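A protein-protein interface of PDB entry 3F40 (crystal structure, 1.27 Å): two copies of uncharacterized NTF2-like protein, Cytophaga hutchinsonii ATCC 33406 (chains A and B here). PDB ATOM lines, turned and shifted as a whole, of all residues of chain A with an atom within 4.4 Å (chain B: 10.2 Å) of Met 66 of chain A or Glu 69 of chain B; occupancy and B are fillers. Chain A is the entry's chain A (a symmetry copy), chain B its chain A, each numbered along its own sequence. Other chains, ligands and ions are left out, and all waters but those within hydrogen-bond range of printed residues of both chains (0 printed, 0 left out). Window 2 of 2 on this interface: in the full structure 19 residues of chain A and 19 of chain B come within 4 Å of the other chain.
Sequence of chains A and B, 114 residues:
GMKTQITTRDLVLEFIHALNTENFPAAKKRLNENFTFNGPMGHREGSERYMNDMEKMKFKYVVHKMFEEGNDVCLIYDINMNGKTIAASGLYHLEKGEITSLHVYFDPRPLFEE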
ATOM      1  N   ARG A   9      24.731  26.132 -11.607  1.00  0.00           N
ATOM      2  CA  ARG A   9      24.420  24.716 -11.920  1.00  0.00           C
ATOM      3  C   ARG A   9      25.111  23.793 -10.930  1.00  0.00           C
ATOM      4  O   ARG A   9      24.562  22.782 -10.482  1.00  0.00           O
ATOM      5  CB  ARG A   9      24.800  24.358 -13.363  1.00  0.00           C
ATOM      6  CG  ARG A   9      23.873  24.961 -14.413  1.00  0.00           C
ATOM      7  N   VAL A  12      23.059  23.778  -7.597  1.00  0.00           N
ATOM      8  CA  VAL A  12      21.897  22.906  -7.562  1.00  0.00           C
ATOM      9  C   VAL A  12      22.317  21.451  -7.453  1.00  0.00           C
ATOM     10  O   VAL A  12      21.757  20.680  -6.663  1.00  0.00           O
ATOM     11  CB  VAL A  12      20.941  23.149  -8.753  1.00  0.00           C
ATOM     12  CG1 VAL A  12      19.826  22.127  -8.776  1.00  0.00           C
ATOM     13  CG2 VAL A  12      20.388  24.602  -8.693  1.00  0.00           C
ATOM     14  N   LEU A  13      23.319  21.068  -8.225  1.00  0.00           N
ATOM     15  CA  LEU A  13      23.768  19.673  -8.166  1.00  0.00           C
ATOM     16  C   LEU A  13      24.372  19.330  -6.810  1.00  0.00           C
ATOM     17  O   LEU A  13      24.249  18.188  -6.354  1.00  0.00           O
ATOM     18  CB  LEU A  13      24.713  19.373  -9.317  1.00  0.00           C
ATOM     19  CG  LEU A  13      23.994  19.385 -10.655  1.00  0.00           C
ATOM     20  CD1 LEU A  13      24.966  18.992 -11.790  1.00  0.00           C
ATOM     21  CD2 LEU A  13      22.748  18.479 -10.692  1.00  0.00           C
ATOM     22  N   LYS A  65      17.628  14.868 -16.415  1.00  0.00           N
ATOM     23  CA  LYS A  65      17.876  16.033 -17.283  1.00  0.00           C
ATOM     24  C   LYS A  65      17.982  17.263 -16.442  1.00  0.00           C
ATOM     25  O   LYS A  65      17.341  17.371 -15.398  1.00  0.00           O
ATOM     26  CB  LYS A  65      16.755  16.218 -18.302  1.00  0.00           C
ATOM     27  CG  LYS A  65      16.577  15.054 -19.230  1.00  0.00           C
ATOM     28  CD  LYS A  65      15.364  15.234 -20.110  1.00  0.00           C
ATOM     29  CE  LYS A  65      15.052  13.976 -20.945  1.00  0.00           C
ATOM     30  NZ  LYS A  65      16.010  13.693 -22.040  1.00  0.00           N
ATOM     31  N   MET A  66      18.819  18.178 -16.896  1.00  0.00           N
ATOM     32  CA  MET A  66      19.003  19.454 -16.239  1.00  0.00           C
ATOM     33  C   MET A  66      18.978  20.544 -17.278  1.00  0.00           C
ATOM     34  O   MET A  66      19.639  20.444 -18.333  1.00  0.00           O
ATOM     35  CB  MET A  66      20.329  19.452 -15.507  1.00  0.00           C
ATOM     36  CG  MET A  66      20.670  20.756 -14.843  1.00  0.00           C
ATOM     37  SD  MET A  66      22.196  20.531 -13.756  1.00  0.00           S
ATOM     38  CE  MET A  66      21.879  21.958 -12.649  1.00  0.00           C
ATOM     39  N   PHE A  67      18.239  21.588 -16.956  1.00  0.00           N
ATOM     40  CA  PHE A  67      18.123  22.770 -17.768  1.00  0.00           C
ATOM     41  C   PHE A  67      18.472  24.001 -16.964  1.00  0.00           C
ATOM     42  O   PHE A  67      18.248  24.051 -15.768  1.00  0.00           O
ATOM     43  CB  PHE A  67      16.681  23.000 -18.273  1.00  0.00           C
ATOM     44  CG  PHE A  67      16.098  21.855 -19.012  1.00  0.00           C
ATOM     45  CD1 PHE A  67      15.466  20.826 -18.365  1.00  0.00           C
ATOM     46  CD2 PHE A  67      16.099  21.860 -20.404  1.00  0.00           C
ATOM     47  CE1 PHE A  67      14.894  19.791 -19.073  1.00  0.00           C
ATOM     48  CE2 PHE A  67      15.526  20.820 -21.118  1.00  0.00           C
ATOM     49  CZ  PHE A  67      14.941  19.777 -20.440  1.00  0.00           C
ATOM     50  N   VAL A  73      16.926  26.998 -12.702  1.00  0.00           N
ATOM     51  CA  VAL A  73      17.347  25.655 -13.059  1.00  0.00           C
ATOM     52  C   VAL A  73      16.160  24.726 -12.935  1.00  0.00           C
ATOM     53  O   VAL A  73      15.432  24.772 -11.954  1.00  0.00           O
ATOM     54  CB  VAL A  73      18.538  25.163 -12.168  1.00  0.00           C
ATOM     55  CG1 VAL A  73      18.805  23.656 -12.372  1.00  0.00           C
ATOM     56  CG2 VAL A  73      19.770  26.007 -12.448  1.00  0.00           C
ATOM     57  N   CYS A  74      15.932  23.907 -13.952  1.00  0.00           N
ATOM     58  CA  CYS A  74      14.877  22.900 -13.875  1.00  0.00           C
ATOM     59  C   CYS A  74      15.441  21.500 -14.039  1.00  0.00           C
ATOM     60  O   CYS A  74      16.088  21.185 -15.034  1.00  0.00           O
ATOM     61  CB  CYS A  74      13.782  23.164 -14.918  1.00  0.00           C
ATOM     62  SG  CYS A  74      12.237  22.288 -14.537  1.00  0.00           S
ATOM     63  N   LEU A  75      15.150  20.663 -13.052  1.00  0.00           N
ATOM     64  CA  LEU A  75      15.578  19.275 -13.051  1.00  0.00           C
ATOM     65  C   LEU A  75      14.414  18.362 -13.365  1.00  0.00           C
ATOM     66  O   LEU A  75      13.318  18.538 -12.851  1.00  0.00           O
ATOM     67  CB  LEU A  75      16.143  18.848 -11.687  1.00  0.00           C
ATOM     68  CG  LEU A  75      17.330  19.666 -11.155  1.00  0.00           C
ATOM     69  CD1 LEU A  75      17.820  19.095  -9.793  1.00  0.00           C
ATOM     70  CD2 LEU A  75      18.465  19.743 -12.126  1.00  0.00           C
ATOM     71  N   THR B   8      14.205  24.583 -33.056  1.00  0.00           N
ATOM     72  CA  THR B   8      13.421  23.675 -32.199  1.00  0.00           C
ATOM     73  C   THR B   8      12.607  24.454 -31.147  1.00  0.00           C
ATOM     74  O   THR B   8      11.521  24.025 -30.737  1.00  0.00           O
ATOM     75  CB  THR B   8      14.332  22.617 -31.565  1.00  0.00           C
ATOM     76  OG1 THR B   8      15.483  23.269 -31.078  1.00  0.00           O
ATOM     77  CG2 THR B   8      14.793  21.684 -32.582  1.00  0.00           C
ATOM     78  N   ARG B   9      13.117  25.612 -30.726  1.00  0.00           N
ATOM     79  CA  ARG B   9      12.374  26.453 -29.757  1.00  0.00           C
ATOM     80  C   ARG B   9      11.174  27.099 -30.431  1.00  0.00           C
ATOM     81  O   ARG B   9      10.086  27.218 -29.860  1.00  0.00           O
ATOM     82  CB  ARG B   9      13.280  27.511 -29.114  1.00  0.00           C
ATOM     83  CG  ARG B   9      14.272  26.944 -28.105  1.00  0.00           C
ATOM     84  N   VAL B  12       8.317  24.438 -30.708  1.00  0.00           N
ATOM     85  CA  VAL B  12       7.509  24.237 -29.517  1.00  0.00           C
ATOM     86  C   VAL B  12       6.566  25.407 -29.300  1.00  0.00           C
ATOM     87  O   VAL B  12       5.378  25.225 -29.002  1.00  0.00           O
ATOM     88  CB  VAL B  12       8.368  23.941 -28.266  1.00  0.00           C
ATOM     89  CG1 VAL B  12       7.514  23.889 -27.017  1.00  0.00           C
ATOM     90  CG2 VAL B  12       9.160  22.618 -28.475  1.00  0.00           C
ATOM     91  N   MET B  66      10.770  29.065 -20.297  1.00  0.00           N
ATOM     92  CA  MET B  66      11.144  28.093 -21.302  1.00  0.00           C
ATOM     93  C   MET B  66      12.614  27.789 -21.161  1.00  0.00           C
ATOM     94  O   MET B  66      13.452  28.706 -21.040  1.00  0.00           O
ATOM     95  CB  MET B  66      10.851  28.657 -22.677  1.00  0.00           C
ATOM     96  CG  MET B  66      11.268  27.766 -23.812  1.00  0.00           C
ATOM     97  SD  MET B  66      10.605  28.462 -25.436  1.00  0.00           S
ATOM     98  CE  MET B  66      10.651  26.887 -26.375  1.00  0.00           C
ATOM     99  N   PHE B  67      12.912  26.506 -21.209  1.00  0.00           N
ATOM    100  CA  PHE B  67      14.256  25.993 -21.161  1.00  0.00           C
ATOM    101  C   PHE B  67      14.523  25.097 -22.349  1.00  0.00           C
ATOM    102  O   PHE B  67      13.630  24.439 -22.850  1.00  0.00           O
ATOM    103  CB  PHE B  67      14.507  25.114 -19.915  1.00  0.00           C
ATOM    104  CG  PHE B  67      14.203  25.775 -18.625  1.00  0.00           C
ATOM    105  CD1 PHE B  67      12.940  25.772 -18.093  1.00  0.00           C
ATOM    106  CD2 PHE B  67      15.235  26.333 -17.875  1.00  0.00           C
ATOM    107  CE1 PHE B  67      12.686  26.357 -16.870  1.00  0.00           C
ATOM    108  CE2 PHE B  67      14.982  26.923 -16.647  1.00  0.00           C
ATOM    109  CZ  PHE B  67      13.696  26.947 -16.161  1.00  0.00           C
ATOM    110  N   GLU B  68      15.775  25.064 -22.802  1.00  0.00           N
ATOM    111  CA  GLU B  68      16.203  24.100 -23.835  1.00  0.00           C
ATOM    112  C   GLU B  68      17.559  23.515 -23.480  1.00  0.00           C
ATOM    113  O   GLU B  68      18.450  24.201 -22.982  1.00  0.00           O
ATOM    114  CB  GLU B  68      16.320  24.683 -25.264  1.00  0.00           C
ATOM    115  CG  GLU B  68      16.523  23.561 -26.341  1.00  0.00           C
ATOM    116  CD  GLU B  68      16.399  24.049 -27.788  1.00  0.00           C
ATOM    117  OE1 GLU B  68      17.006  25.066 -28.137  1.00  0.00           O
ATOM    118  OE2 GLU B  68      15.677  23.402 -28.581  1.00  0.00           O
ATOM    119  N   GLU B  69      17.687  22.226 -23.757  1.00  0.00           N
ATOM    120  CA  GLU B  69      18.955  21.503 -23.577  1.00  0.00           C
ATOM    121  C   GLU B  69      18.932  20.383 -24.602  1.00  0.00           C
ATOM    122  O   GLU B  69      18.153  19.462 -24.507  1.00  0.00           O
ATOM    123  CB  GLU B  69      19.076  20.977 -22.153  1.00  0.00           C
ATOM    124  CG  GLU B  69      20.416  20.369 -21.798  1.00  0.00           C
ATOM    125  CD  GLU B  69      21.503  21.404 -21.890  1.00  0.00           C
ATOM    126  OE1 GLU B  69      21.413  22.439 -21.191  1.00  0.00           O
ATOM    127  OE2 GLU B  69      22.443  21.180 -22.665  1.00  0.00           O
ATOM    128  N   GLY B  70      19.982  20.251 -25.394  1.00  0.00           N
ATOM    129  CA  GLY B  70      20.027  19.131 -26.330  1.00  0.00           C
ATOM    130  C   GLY B  70      18.690  18.979 -27.074  1.00  0.00           C
ATOM    131  O   GLY B  70      18.163  19.944 -27.590  1.00  0.00           O
ATOM    132  N   ASN B  71      18.106  17.791 -27.104  1.00  0.00           N
ATOM    133  CA  ASN B  71      16.878  17.609 -27.911  1.00  0.00           C
ATOM    134  C   ASN B  71      15.580  17.778 -27.120  1.00  0.00           C
ATOM    135  O   ASN B  71      14.515  17.287 -27.504  1.00  0.00           O
ATOM    136  CB  ASN B  71      16.917  16.272 -28.594  1.00  0.00           C
ATOM    137  CG  ASN B  71      18.020  16.222 -29.646  1.00  0.00           C
ATOM    138  OD1 ASN B  71      18.327  17.237 -30.288  1.00  0.00           O
ATOM    139  ND2 ASN B  71      18.658  15.072 -29.778  1.00  0.00           N
ATOM    140  N   ASP B  72      15.691  18.490 -26.011  1.00  0.00           N
ATOM    141  CA  ASP B  72      14.566  18.681 -25.103  1.00  0.00           C
ATOM    142  C   ASP B  72      14.310  20.144 -24.822  1.00  0.00           C
ATOM    143  O   ASP B  72      15.209  20.945 -24.665  1.00  0.00           O
ATOM    144  CB  ASP B  72      14.784  17.990 -23.764  1.00  0.00           C
ATOM    145  CG  ASP B  72      15.011  16.498 -23.928  1.00  0.00           C
ATOM    146  OD1 ASP B  72      14.083  15.840 -24.403  1.00  0.00           O
ATOM    147  OD2 ASP B  72      16.091  15.991 -23.578  1.00  0.00           O
ATOM    148  N   VAL B  73      13.023  20.441 -24.715  1.00  0.00           N
ATOM    149  CA  VAL B  73      12.497  21.727 -24.293  1.00  0.00           C
ATOM    150  C   VAL B  73      11.582  21.509 -23.109  1.00  0.00           C
ATOM    151  O   VAL B  73      10.750  20.614 -23.119  1.00  0.00           O
ATOM    152  CB  VAL B  73      11.743  22.457 -25.457  1.00  0.00           C
ATOM    153  CG1 VAL B  73      10.969  23.688 -24.936  1.00  0.00           C
ATOM    154  CG2 VAL B  73      12.728  22.820 -26.556  1.00  0.00           C
ATOM    155  N   CYS B  74      11.761  22.302 -22.061  1.00  0.00           N
ATOM    156  CA  CYS B  74      10.855  22.240 -20.918  1.00  0.00           C
ATOM    157  C   CYS B  74      10.175  23.577 -20.682  1.00  0.00           C
ATOM    158  O   CYS B  74      10.828  24.600 -20.496  1.00  0.00           O
ATOM    159  CB  CYS B  74      11.590  21.780 -19.651  1.00  0.00           C
ATOM    160  SG  CYS B  74      10.452  21.194 -18.363  1.00  0.00           S
ATOM    161  N   LEU B  75       8.850  23.534 -20.663  1.00  0.00           N
ATOM    162  CA  LEU B  75       8.031  24.708 -20.421  1.00  0.00           C
ATOM    163  C   LEU B  75       7.454  24.673 -19.023  1.00  0.00           C
ATOM    164  O   LEU B  75       6.982  23.642 -18.562  1.00  0.00           O
ATOM    165  CB  LEU B  75       6.852  24.801 -21.403  1.00  0.00           C
ATOM    166  CG  LEU B  75       7.212  24.826 -22.897  1.00  0.00           C
ATOM    167  CD1 LEU B  75       5.928  24.963 -23.765  1.00  0.00           C
ATOM    168  CD2 LEU B  75       8.191  25.902 -23.243  1.00  0.00           C
ATOM    169  N   LEU B  91       7.626  18.661 -20.648  1.00  0.00           N
ATOM    170  CA  LEU B  91       8.900  18.253 -21.224  1.00  0.00           C
ATOM    171  C   LEU B  91       8.654  17.695 -22.627  1.00  0.00           C
ATOM    172  O   LEU B  91       8.009  16.662 -22.803  1.00  0.00           O
ATOM    173  CB  LEU B  91       9.533  17.190 -20.344  1.00  0.00           C
ATOM    174  CG  LEU B  91      10.826  16.577 -20.833  1.00  0.00           C
ATOM    175  CD1 LEU B  91      11.962  17.597 -20.873  1.00  0.00           C
ATOM    176  CD2 LEU B  91      11.184  15.380 -19.934  1.00  0.00           C
ATOM    177  N   TYR B  92       9.131  18.433 -23.627  1.00  0.00           N
ATOM    178  CA  TYR B  92       8.968  18.113 -25.033  1.00  0.00           C
ATOM    179  C   TYR B  92      10.290  17.603 -25.594  1.00  0.00           C
ATOM    180  O   TYR B  92      11.330  18.271 -25.434  1.00  0.00           O
ATOM    181  CB  TYR B  92       8.527  19.370 -25.820  1.00  0.00           C
ATOM    182  CG  TYR B  92       7.227  19.957 -25.382  1.00  0.00           C
ATOM    183  CD1 TYR B  92       7.138  20.742 -24.248  1.00  0.00           C
ATOM    184  CD2 TYR B  92       6.086  19.756 -26.104  1.00  0.00           C
ATOM    185  CE1 TYR B  92       5.917  21.229 -23.809  1.00  0.00           C
ATOM    186  CE2 TYR B  92       4.852  20.239 -25.662  1.00  0.00           C
ATOM    187  CZ  TYR B  92       4.775  20.960 -24.501  1.00  0.00           C
ATOM    188  OH  TYR B  92       3.569  21.424 -24.037  1.00  0.00           O
ATOM    189  N   HIS B  93      10.234  16.461 -26.278  1.00  0.00           N
ATOM    190  CA  HIS B  93      11.416  15.926 -26.955  1.00  0.00           C
ATOM    191  C   HIS B  93      11.225  16.105 -28.462  1.00  0.00           C
ATOM    192  O   HIS B  93      10.132  15.846 -28.972  1.00  0.00           O
ATOM    193  CB  HIS B  93      11.605  14.442 -26.636  1.00  0.00           C
ATOM    194  CG  HIS B  93      12.895  13.887 -27.129  1.00  0.00           C
ATOM    195  ND1 HIS B  93      14.088  14.121 -26.486  1.00  0.00           N
ATOM    196  CD2 HIS B  93      13.177  13.095 -28.196  1.00  0.00           C
ATOM    197  CE1 HIS B  93      15.057  13.500 -27.144  1.00  0.00           C
ATOM    198  NE2 HIS B  93      14.532  12.904 -28.202  1.00  0.00           N
ATOM    199  N   LEU B  94      12.283  16.528 -29.122  1.00  0.00           N
ATOM    200  CA  LEU B  94      12.253  16.778 -30.578  1.00  0.00           C
ATOM    201  C   LEU B  94      13.332  16.005 -31.265  1.00  0.00           C
ATOM    202  O   LEU B  94      14.481  15.888 -30.789  1.00  0.00           O
ATOM    203  CB  LEU B  94      12.439  18.266 -30.852  1.00  0.00           C
ATOM    204  CG  LEU B  94      11.299  19.117 -30.223  1.00  0.00           C
ATOM    205  CD1 LEU B  94      11.739  19.702 -28.894  1.00  0.00           C
ATOM    206  CD2 LEU B  94      10.789  20.227 -31.158  1.00  0.00           C
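The side-chain amino group of Lys 65 of chain A is in salt-bridge range of the side-chain carboxylate of Asp 72 of chain B.
The side-chain hydroxyl (OG1) of Thr 8 of chain B lies within hydrogen-bond range of the side-chain carboxylate (OE2) of Glu 68 of chain B (2.5 Å). The backbone NH of Phe 67 of chain B is in hydrogen-bond range of the backbone carbonyl oxygen of Cys 74 of chain B (2.9 Å). OD1 of Asp 72 of chain B sits at hydrogen-bond distance from ND1 of His 93 of chain B, 2.7 Å away. The backbone NH (N) of Phe 67 of chain A is in hydrogen-bond range of the backbone carbonyl oxygen (O) of Cys 74 of chain A (2.9 Å).
O of Met 66 of chain A touches CG of Glu 69 of chain B (3.6 Å). Phe 67 of chain A touches Phe 67 of chain B. Glu 68 of chain B touches Phe 67 of chain A (C to CD2, 3.8 Å). Phe 67 of chain A touches Glu 69 of chain B. Phe 67 of chain A touches Asp 72 of chain B (CE2 to O, 3.6 Å). CB of Cys 74 of chain B touches CE1 of Phe 67 of chain A, 3.9 Å away. Leu 91 of chain B touches Phe 67 of chain A (CD1 to CZ, 3.7 Å). Phe 67 of chain B touches Cys 74 of chain A (CE1 to CB, 3.9 Å).
Printed residues of chain B within 4 Å of Lys 65 of chain A: Asp 72 (2.8 Å). Met 66 of chain A touches one residue of chain B. Printed residues of chain A within 4 Å of Phe 67 of chain B: Phe 67 and Cys 74. Glu 69 of chain B touches just these residues of chain A: Met 66 and Phe 67. Gly 70 of chain B touches none of the printed residues of chain A. Of the printed residues of chain A, Cys 74 of chain B touches Phe 67. His 93 of chain B touches none of the printed residues of chain A.
Printed residues of chain A that touch a printed residue of chain B: Lys 65, Met 66, Phe 67 and Cys 74. Hydrophobic or aromatic side chains of chain A within 4 Å of the printed part of chain B: Phe 67. Printed residues of chain B that touch a printed residue of chain A: Phe 67, Glu 68, Glu 69, Asp 72, Cys 74 and Leu 91. Hydrophobic or aromatic side chains of chain B that line the printed part of chain A: Phe 67 and Leu 91. Among the printed residues, 9 pairs touch across the chains. Among the printed residues, Asp or Glu carboxylates within 4 Å of a Lys or Arg side-chain nitrogen of the other chain: Lys 65 of chain A with Asp 72 of chain B.
Phe 67 of chain B touches its own counterpart, Phe 67 of chain A. Phe 67 of chain A touches Cys 74 of chain B, and with the chains exchanged Cys 74 of chain A touches Phe 67 of chain B. Of the 9 pairs that touch across the chains among the printed residues, 3 have their exchanged pair printed and touching as well.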
